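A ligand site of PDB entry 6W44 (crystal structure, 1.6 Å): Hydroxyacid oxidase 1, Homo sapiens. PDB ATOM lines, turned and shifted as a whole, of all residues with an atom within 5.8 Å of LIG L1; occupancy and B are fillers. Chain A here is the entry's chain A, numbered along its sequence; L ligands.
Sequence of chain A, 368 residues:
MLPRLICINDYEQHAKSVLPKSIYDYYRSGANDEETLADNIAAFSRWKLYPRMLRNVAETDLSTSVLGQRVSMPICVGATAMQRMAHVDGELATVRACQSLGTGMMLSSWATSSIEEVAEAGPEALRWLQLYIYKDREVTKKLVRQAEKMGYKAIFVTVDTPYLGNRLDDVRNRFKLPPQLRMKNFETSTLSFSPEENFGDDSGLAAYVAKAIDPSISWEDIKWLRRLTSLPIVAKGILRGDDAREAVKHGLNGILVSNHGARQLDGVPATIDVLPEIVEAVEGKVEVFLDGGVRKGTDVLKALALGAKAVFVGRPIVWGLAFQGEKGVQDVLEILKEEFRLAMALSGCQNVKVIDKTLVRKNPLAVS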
ATOM      1  N   SER A  22       2.405 -28.179  15.582  1.00  0.00           N
ATOM      2  CA  SER A  22       3.508 -27.422  14.926  1.00  0.00           C
ATOM      3  C   SER A  22       3.850 -26.158  15.728  1.00  0.00           C
ATOM      4  O   SER A  22       5.039 -25.791  15.796  1.00  0.00           O
ATOM      5  CB  SER A  22       3.161 -27.094  13.501  1.00  0.00           C
ATOM      6  OG  SER A  22       2.055 -26.217  13.444  1.00  0.00           O
ATOM      7  N   ILE A  23       2.861 -25.512  16.354  1.00  0.00           N
ATOM      8  CA  ILE A  23       3.037 -24.259  17.109  1.00  0.00           C
ATOM      9  C   ILE A  23       3.634 -24.596  18.484  1.00  0.00           C
ATOM     10  O   ILE A  23       4.631 -23.930  18.838  1.00  0.00           O
ATOM     11  CB  ILE A  23       1.698 -23.490  17.208  1.00  0.00           C
ATOM     12  CG1 ILE A  23       1.213 -23.057  15.816  1.00  0.00           C
ATOM     13  CG2 ILE A  23       1.836 -22.327  18.139  1.00  0.00           C
ATOM     14  CD1 ILE A  23      -0.165 -22.427  15.859  1.00  0.00           C
ATOM     15  N   TYR A  26       7.284 -25.467  17.896  1.00  0.00           N
ATOM     16  CA  TYR A  26       8.056 -24.227  17.615  1.00  0.00           C
ATOM     17  C   TYR A  26       8.462 -23.577  18.941  1.00  0.00           C
ATOM     18  O   TYR A  26       9.655 -23.239  19.186  1.00  0.00           O
ATOM     19  CB  TYR A  26       7.286 -23.231  16.738  1.00  0.00           C
ATOM     20  CG  TYR A  26       7.927 -21.874  16.787  1.00  0.00           C
ATOM     21  CD1 TYR A  26       9.129 -21.614  16.152  1.00  0.00           C
ATOM     22  CD2 TYR A  26       7.355 -20.854  17.507  1.00  0.00           C
ATOM     23  CE1 TYR A  26       9.742 -20.381  16.278  1.00  0.00           C
ATOM     24  CE2 TYR A  26       7.920 -19.598  17.576  1.00  0.00           C
ATOM     25  CZ  TYR A  26       9.139 -19.368  16.994  1.00  0.00           C
ATOM     26  OH  TYR A  26       9.694 -18.140  17.183  1.00  0.00           O
ATOM     27  N   ALA A  81       9.310 -13.952  19.824  1.00  0.00           N
ATOM     28  CA  ALA A  81       8.627 -13.649  18.558  1.00  0.00           C
ATOM     29  C   ALA A  81       7.311 -14.427  18.551  1.00  0.00           C
ATOM     30  O   ALA A  81       7.205 -15.490  19.176  1.00  0.00           O
ATOM     31  CB  ALA A  81       9.497 -14.031  17.388  1.00  0.00           C
ATOM     32  N   MET A  82       6.341 -13.926  17.848  1.00  0.00           N
ATOM     33  CA  MET A  82       5.181 -14.714  17.340  1.00  0.00           C
ATOM     34  C   MET A  82       4.196 -14.975  18.479  1.00  0.00           C
ATOM     35  O   MET A  82       3.592 -16.092  18.480  1.00  0.00           O
ATOM     36  CB  MET A  82       5.581 -16.074  16.737  1.00  0.00           C
ATOM     37  CG  MET A  82       6.600 -16.018  15.593  1.00  0.00           C
ATOM     38  SD  MET A  82       6.154 -14.972  14.166  1.00  0.00           S
ATOM     39  CE  MET A  82       4.427 -15.403  14.007  1.00  0.00           C
ATOM     40  N   MET A  85       0.531 -16.125  17.771  1.00  0.00           N
ATOM     41  CA  MET A  85       0.236 -17.563  17.490  1.00  0.00           C
ATOM     42  C   MET A  85      -0.226 -18.296  18.744  1.00  0.00           C
ATOM     43  O   MET A  85      -0.818 -19.392  18.601  1.00  0.00           O
ATOM     44  CB  MET A  85       1.459 -18.241  16.880  1.00  0.00           C
ATOM     45  CG  MET A  85       1.936 -17.516  15.660  1.00  0.00           C
ATOM     46  SD  MET A  85       0.683 -17.586  14.357  1.00  0.00           S
ATOM     47  CE  MET A  85       0.948 -15.992  13.558  1.00  0.00           C
ATOM     48  N   SER A 108      10.102  -8.157  21.417  1.00  0.00           N
ATOM     49  CA  SER A 108      10.893  -8.713  20.306  1.00  0.00           C
ATOM     50  C   SER A 108      10.893  -7.696  19.168  1.00  0.00           C
ATOM     51  O   SER A 108       9.890  -7.124  18.908  1.00  0.00           O
ATOM     52  CB  SER A 108      10.281  -9.986  19.808  1.00  0.00           C
ATOM     53  OG  SER A 108      10.903 -10.405  18.620  1.00  0.00           O
ATOM     54  N   TRP A 110      10.808  -8.736  16.179  1.00  0.00           N
ATOM     55  CA  TRP A 110       9.862  -9.403  15.249  1.00  0.00           C
ATOM     56  C   TRP A 110       8.489  -9.542  15.923  1.00  0.00           C
ATOM     57  O   TRP A 110       7.889 -10.587  15.734  1.00  0.00           O
ATOM     58  CB  TRP A 110      10.397 -10.765  14.816  1.00  0.00           C
ATOM     59  CG  TRP A 110      11.503 -10.688  13.815  1.00  0.00           C
ATOM     60  CD1 TRP A 110      12.830 -10.553  14.100  1.00  0.00           C
ATOM     61  CD2 TRP A 110      11.407 -10.788  12.388  1.00  0.00           C
ATOM     62  NE1 TRP A 110      13.559 -10.555  12.952  1.00  0.00           N
ATOM     63  CE2 TRP A 110      12.714 -10.697  11.880  1.00  0.00           C
ATOM     64  CE3 TRP A 110      10.347 -10.943  11.486  1.00  0.00           C
ATOM     65  CZ2 TRP A 110      12.994 -10.742  10.514  1.00  0.00           C
ATOM     66  CZ3 TRP A 110      10.622 -10.990  10.134  1.00  0.00           C
ATOM     67  CH2 TRP A 110      11.924 -10.893   9.663  1.00  0.00           C
ATOM     68  N   TYR A 132      17.687  -6.713  16.689  1.00  0.00           N
ATOM     69  CA  TYR A 132      18.700  -7.370  15.836  1.00  0.00           C
ATOM     70  C   TYR A 132      19.282  -6.258  14.964  1.00  0.00           C
ATOM     71  O   TYR A 132      18.492  -5.311  14.591  1.00  0.00           O
ATOM     72  CB  TYR A 132      18.099  -8.433  14.923  1.00  0.00           C
ATOM     73  CG  TYR A 132      17.686  -9.682  15.662  1.00  0.00           C
ATOM     74  CD1 TYR A 132      18.679 -10.503  16.142  1.00  0.00           C
ATOM     75  CD2 TYR A 132      16.366 -10.058  15.813  1.00  0.00           C
ATOM     76  CE1 TYR A 132      18.354 -11.677  16.800  1.00  0.00           C
ATOM     77  CE2 TYR A 132      16.022 -11.225  16.481  1.00  0.00           C
ATOM     78  CZ  TYR A 132      17.033 -12.045  16.945  1.00  0.00           C
ATOM     79  OH  TYR A 132      16.767 -13.220  17.637  1.00  0.00           O
ATOM     80  N   THR A 161      22.948 -14.475  17.322  1.00  0.00           N
ATOM     81  CA  THR A 161      22.140 -14.939  16.174  1.00  0.00           C
ATOM     82  C   THR A 161      22.646 -14.357  14.851  1.00  0.00           C
ATOM     83  O   THR A 161      21.911 -13.667  14.215  1.00  0.00           O
ATOM     84  CB  THR A 161      20.652 -14.647  16.414  1.00  0.00           C
ATOM     85  OG1 THR A 161      20.358 -15.131  17.708  1.00  0.00           O
ATOM     86  CG2 THR A 161      19.721 -15.298  15.424  1.00  0.00           C
ATOM     87  N   LEU A 164      20.000 -18.181  12.263  1.00  0.00           N
ATOM     88  CA  LEU A 164      19.082 -18.844  13.203  1.00  0.00           C
ATOM     89  C   LEU A 164      19.541 -20.282  13.447  1.00  0.00           C
ATOM     90  O   LEU A 164      20.009 -20.920  12.535  1.00  0.00           O
ATOM     91  CB  LEU A 164      17.666 -18.827  12.620  1.00  0.00           C
ATOM     92  CG  LEU A 164      16.747 -17.681  13.069  1.00  0.00           C
ATOM     93  CD1 LEU A 164      15.374 -17.872  12.460  1.00  0.00           C
ATOM     94  CD2 LEU A 164      16.599 -17.584  14.575  1.00  0.00           C
ATOM     95  N   ARG A 167      16.485 -25.945  14.672  1.00  0.00           N
ATOM     96  CA  ARG A 167      15.492 -26.654  15.528  1.00  0.00           C
ATOM     97  C   ARG A 167      14.886 -27.743  14.632  1.00  0.00           C
ATOM     98  O   ARG A 167      14.105 -27.393  13.764  1.00  0.00           O
ATOM     99  CB  ARG A 167      14.548 -25.629  16.161  1.00  0.00           C
ATOM    100  CG  ARG A 167      15.263 -24.479  16.853  1.00  0.00           C
ATOM    101  CD  ARG A 167      15.391 -23.223  15.988  1.00  0.00           C
ATOM    102  NE  ARG A 167      16.133 -22.067  16.517  1.00  0.00           N
ATOM    103  CZ  ARG A 167      15.567 -20.902  16.797  1.00  0.00           C
ATOM    104  NH1 ARG A 167      16.291 -19.905  17.273  1.00  0.00           N
ATOM    105  NH2 ARG A 167      14.269 -20.762  16.601  1.00  0.00           N
ATOM    106  N   ASP A 170      10.988 -27.800  13.578  1.00  0.00           N
ATOM    107  CA  ASP A 170      10.581 -26.718  12.635  1.00  0.00           C
ATOM    108  C   ASP A 170      10.835 -27.180  11.203  1.00  0.00           C
ATOM    109  O   ASP A 170      10.067 -26.792  10.314  1.00  0.00           O
ATOM    110  CB  ASP A 170      11.323 -25.404  12.874  1.00  0.00           C
ATOM    111  CG  ASP A 170      10.848 -24.690  14.125  1.00  0.00           C
ATOM    112  OD1 ASP A 170       9.763 -25.073  14.650  1.00  0.00           O
ATOM    113  OD2 ASP A 170      11.577 -23.762  14.585  1.00  0.00           O
ATOM    114  N   LEU A 205       8.918 -18.687   6.902  1.00  0.00           N
ATOM    115  CA  LEU A 205       9.237 -17.678   7.964  1.00  0.00           C
ATOM    116  C   LEU A 205      10.757 -17.667   8.187  1.00  0.00           C
ATOM    117  O   LEU A 205      11.341 -16.568   8.080  1.00  0.00           O
ATOM    118  CB  LEU A 205       8.444 -18.024   9.234  1.00  0.00           C
ATOM    119  CG  LEU A 205       7.916 -16.877  10.100  1.00  0.00           C
ATOM    120  CD1 LEU A 205       7.614 -15.608   9.317  1.00  0.00           C
ATOM    121  CD2 LEU A 205       6.680 -17.336  10.865  1.00  0.00           C
ATOM    122  N   ALA A 206      11.371 -18.829   8.441  1.00  0.00           N
ATOM    123  CA  ALA A 206      12.806 -18.948   8.804  1.00  0.00           C
ATOM    124  C   ALA A 206      13.664 -18.363   7.668  1.00  0.00           C
ATOM    125  O   ALA A 206      14.696 -17.719   7.962  1.00  0.00           O
ATOM    126  CB  ALA A 206      13.179 -20.382   9.111  1.00  0.00           C
ATOM    127  N   VAL A 209      13.413 -14.574   7.843  1.00  0.00           N
ATOM    128  CA  VAL A 209      14.301 -14.102   8.957  1.00  0.00           C
ATOM    129  C   VAL A 209      15.781 -14.177   8.524  1.00  0.00           C
ATOM    130  O   VAL A 209      16.528 -13.216   8.776  1.00  0.00           O
ATOM    131  CB  VAL A 209      14.032 -14.882  10.265  1.00  0.00           C
ATOM    132  CG1 VAL A 209      14.994 -14.452  11.366  1.00  0.00           C
ATOM    133  CG2 VAL A 209      12.593 -14.715  10.718  1.00  0.00           C
ATOM    134  N   HIS A 260      19.829 -18.136  24.340  1.00  0.00           N
ATOM    135  CA  HIS A 260      18.669 -17.976  23.410  1.00  0.00           C
ATOM    136  C   HIS A 260      17.678 -19.097  23.707  1.00  0.00           C
ATOM    137  O   HIS A 260      17.080 -19.676  22.744  1.00  0.00           O
ATOM    138  CB  HIS A 260      19.120 -17.952  21.944  1.00  0.00           C
ATOM    139  CG  HIS A 260      18.234 -17.181  21.048  1.00  0.00           C
ATOM    140  ND1 HIS A 260      18.642 -15.990  20.456  1.00  0.00           N
ATOM    141  CD2 HIS A 260      16.987 -17.459  20.533  1.00  0.00           C
ATOM    142  CE1 HIS A 260      17.665 -15.564  19.627  1.00  0.00           C
ATOM    143  NE2 HIS A 260      16.654 -16.419  19.666  1.00  0.00           N
ATOM    144  N   ARG A 263      18.234 -22.477  21.765  1.00  0.00           N
ATOM    145  CA  ARG A 263      17.684 -22.567  20.391  1.00  0.00           C
ATOM    146  C   ARG A 263      18.738 -22.248  19.336  1.00  0.00           C
ATOM    147  O   ARG A 263      18.423 -22.338  18.149  1.00  0.00           O
ATOM    148  CB  ARG A 263      16.473 -21.648  20.277  1.00  0.00           C
ATOM    149  CG  ARG A 263      15.331 -22.075  21.182  1.00  0.00           C
ATOM    150  CD  ARG A 263      14.300 -20.970  21.334  1.00  0.00           C
ATOM    151  NE  ARG A 263      13.506 -20.683  20.159  1.00  0.00           N
ATOM    152  CZ  ARG A 263      12.371 -21.331  19.861  1.00  0.00           C
ATOM    153  NH1 ARG A 263      11.997 -22.386  20.553  1.00  0.00           N
ATOM    154  NH2 ARG A 263      11.614 -20.891  18.879  1.00  0.00           N
ATOM    155  N   GLN A 264      19.948 -21.870  19.727  1.00  0.00           N
ATOM    156  CA  GLN A 264      20.986 -21.408  18.772  1.00  0.00           C
ATOM    157  C   GLN A 264      22.029 -22.532  18.673  1.00  0.00           C
ATOM    158  O   GLN A 264      21.817 -23.470  17.911  1.00  0.00           O
ATOM    159  CB  GLN A 264      21.534 -20.034  19.183  1.00  0.00           C
ATOM    160  CG  GLN A 264      20.521 -18.928  18.869  1.00  0.00           C
ATOM    161  CD  GLN A 264      20.297 -18.792  17.378  1.00  0.00           C
ATOM    162  OE1 GLN A 264      19.228 -19.147  16.870  1.00  0.00           O
ATOM    163  NE2 GLN A 264      21.343 -18.397  16.663  1.00  0.00           N
HETATM  164  C1  LIG L   1       5.916 -19.607  14.318  1.00  0.00           C
HETATM  165  C2  LIG L   1       7.101 -19.988  13.608  1.00  0.00           C
HETATM  166  C3  LIG L   1       9.162 -18.949  13.113  1.00  0.00           C
HETATM  167  C4  LIG L   1       9.998 -17.787  13.216  1.00  0.00           C
HETATM  168  C5  LIG L   1       9.507 -16.544  13.899  1.00  0.00           C
HETATM  169  C6  LIG L   1       9.864 -14.265  12.839  1.00  0.00           C
HETATM  170  C7  LIG L   1      11.428 -15.145  14.587  1.00  0.00           C
HETATM  171  C8  LIG L   1      11.822 -16.139  15.480  1.00  0.00           C
HETATM  172  C9  LIG L   1      12.913 -15.875  16.318  1.00  0.00           C
HETATM  173  C10 LIG L   1      13.581 -14.646  16.250  1.00  0.00           C
HETATM  174  C11 LIG L   1      13.592 -16.591  17.337  1.00  0.00           C
HETATM  175  C12 LIG L   1      13.314 -17.931  17.850  1.00  0.00           C
HETATM  176  C13 LIG L   1      13.217 -13.669  15.334  1.00  0.00           C
HETATM  177  O1  LIG L   1      12.364 -18.613  17.426  1.00  0.00           O
HETATM  178  O2  LIG L   1      14.169 -18.394  18.702  1.00  0.00           O
HETATM  179  N1  LIG L   1      14.599 -15.871  17.838  1.00  0.00           N
HETATM  180  N2  LIG L   1      14.570 -14.686  17.189  1.00  0.00           N
HETATM  181  C14 LIG L   1      12.128 -13.948  14.509  1.00  0.00           C
HETATM  182  N3  LIG L   1      10.334 -15.347  13.712  1.00  0.00           N
HETATM  183  C15 LIG L   1      11.265 -17.921  12.676  1.00  0.00           C
HETATM  184  C16 LIG L   1      11.660 -19.124  12.125  1.00  0.00           C
HETATM  185  C17 LIG L   1      10.758 -20.170  12.102  1.00  0.00           C
HETATM  186  N4  LIG L   1       9.508 -20.091  12.580  1.00  0.00           N
HETATM  187  O3  LIG L   1       7.960 -18.830  13.688  1.00  0.00           O
HETATM  188  C18 LIG L   1       4.999 -20.872  14.429  1.00  0.00           C
HETATM  189  N1  LG2 L   2      15.160 -13.713  21.625  1.00  0.00           N
HETATM  190  C1  LG2 L   2      15.318 -12.576  20.893  1.00  0.00           C
HETATM  191  O1  LG2 L   2      16.286 -11.830  21.160  1.00  0.00           O
HETATM  192  N2  LG2 L   2      14.487 -12.220  19.904  1.00  0.00           N
HETATM  193  C2  LG2 L   2      13.429 -12.965  19.563  1.00  0.00           C
HETATM  194  O2  LG2 L   2      12.670 -12.605  18.628  1.00  0.00           O
HETATM  195  C3  LG2 L   2      13.174 -14.221  20.299  1.00  0.00           C
HETATM  196  N3  LG2 L   2      12.126 -15.032  20.018  1.00  0.00           N
HETATM  197  C4  LG2 L   2      11.923 -16.175  20.720  1.00  0.00           C
HETATM  198  C5  LG2 L   2      10.844 -16.994  20.406  1.00  0.00           C
HETATM  199  C6  LG2 L   2      10.634 -18.156  21.118  1.00  0.00           C
HETATM  200  C7  LG2 L   2       9.456 -19.040  20.778  1.00  0.00           C
HETATM  201  C8  LG2 L   2      11.561 -18.551  22.214  1.00  0.00           C
HETATM  202  C9  LG2 L   2      11.322 -19.823  22.990  1.00  0.00           C
HETATM  203  C10 LG2 L   2      12.640 -17.732  22.528  1.00  0.00           C
HETATM  204  C11 LG2 L   2      12.858 -16.566  21.819  1.00  0.00           C
HETATM  205  N4  LG2 L   2      13.953 -15.732  22.133  1.00  0.00           N
HETATM  206  C12 LG2 L   2      14.133 -14.552  21.384  1.00  0.00           C
HETATM  207  C13 LG2 L   2      14.876 -16.097  23.202  1.00  0.00           C
HETATM  208  C14 LG2 L   2      14.370 -15.516  24.520  1.00  0.00           C
HETATM  209  O3  LG2 L   2      14.472 -14.088  24.491  1.00  0.00           O
HETATM  210  C15 LG2 L   2      15.166 -16.070  25.700  1.00  0.00           C
HETATM  211  O4  LG2 L   2      16.558 -16.038  25.382  1.00  0.00           O
HETATM  212  C16 LG2 L   2      14.746 -17.490  26.042  1.00  0.00           C
HETATM  213  O5  LG2 L   2      13.385 -17.698  25.636  1.00  0.00           O
HETATM  214  C17 LG2 L   2      14.886 -17.763  27.529  1.00  0.00           C
HETATM  215  O6  LG2 L   2      14.776 -19.170  27.762  1.00  0.00           O
HETATM  216  P1  LG2 L   2      13.431 -19.786  28.400  1.00  0.00           P
HETATM  217  O7  LG2 L   2      13.026 -18.768  29.451  1.00  0.00           O
HETATM  218  O8  LG2 L   2      13.874 -21.113  28.964  1.00  0.00           O
HETATM  219  O9  LG2 L   2      12.485 -19.884  27.229  1.00  0.00           O
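O of Tyr 26 is in hydrogen-bond range of NH1 of Arg 263 (2.8 Å). The backbone carbonyl oxygen (O) of Arg 263 sits at hydrogen-bond distance from the guanidinium group (NE) of Arg 167 (2.8 Å). A ring nitrogen (ND1) of His 260 sits close to the side-chain hydroxyl (OG1) of Thr 161, 3.4 Å away. NH1 of Arg 167 lies within hydrogen-bond range of OE1 of Gln 264 (3.1 Å). The backbone NH (N) of Trp 110 sits at hydrogen-bond distance from the side-chain hydroxyl (OG) of Ser 108, at 3.0 Å.
The side-chain hydroxyl (OH) of Tyr 132 lies within hydrogen-bond range of a nitrogen (N2) of LIG L1. An oxygen (O1) of LIG L1 is in hydrogen-bond range of the side-chain hydroxyl of Tyr 26 (2.7 Å). An oxygen (O2) of LIG L1 lies within salt-bridge range of the guanidinium group (NE) of Arg 263. A ring nitrogen (NE2) of His 260 is in hydrogen-bond range of a nitrogen (N1) of LIG L1. The guanidinium group (NH1) of Arg 167 lies within salt-bridge range of an oxygen (O2) of LIG L1 (3.0 Å). The side-chain hydroxyl (OH) of Tyr 132 sits at hydrogen-bond distance from a nitrogen (N2) of LG2 L2 (3.4 Å). N3 of LG2 L2 is in hydrogen-bond range of N of Ala 81 (3.0 Å). An oxygen (O2) of LG2 L2 lies within hydrogen-bond range of the side-chain hydroxyl (OG) of Ser 108, 2.8 Å away.
Ala 81 touches LIG L1 (CB to C7, 3.6 Å). Met 82 touches LIG L1 (CG to C5, 3.4 Å). CD1 of Trp 110 touches C13 of LIG L1, at 3.4 Å. CD1 of Leu 164 touches C16 of LIG L1 (3.9 Å). CD2 of Leu 205 touches O3 of LIG L1, 3.4 Å away. Ala 206 touches LIG L1 (CA to C16, 3.5 Å). Val 209 touches LIG L1. Hydrophobic or aromatic side chains that line LIG L1: Tyr 26, Ala 81, Met 82, Trp 110, Tyr 132, Leu 164, Leu 205, Ala 206, Val 209 and His 260. The nearest printed residue that does not touch LIG L1 is Asp 170 (4.4 Å).
N1 of LIG L1 lies close to N3 of LG2 L2 (3.4 Å).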
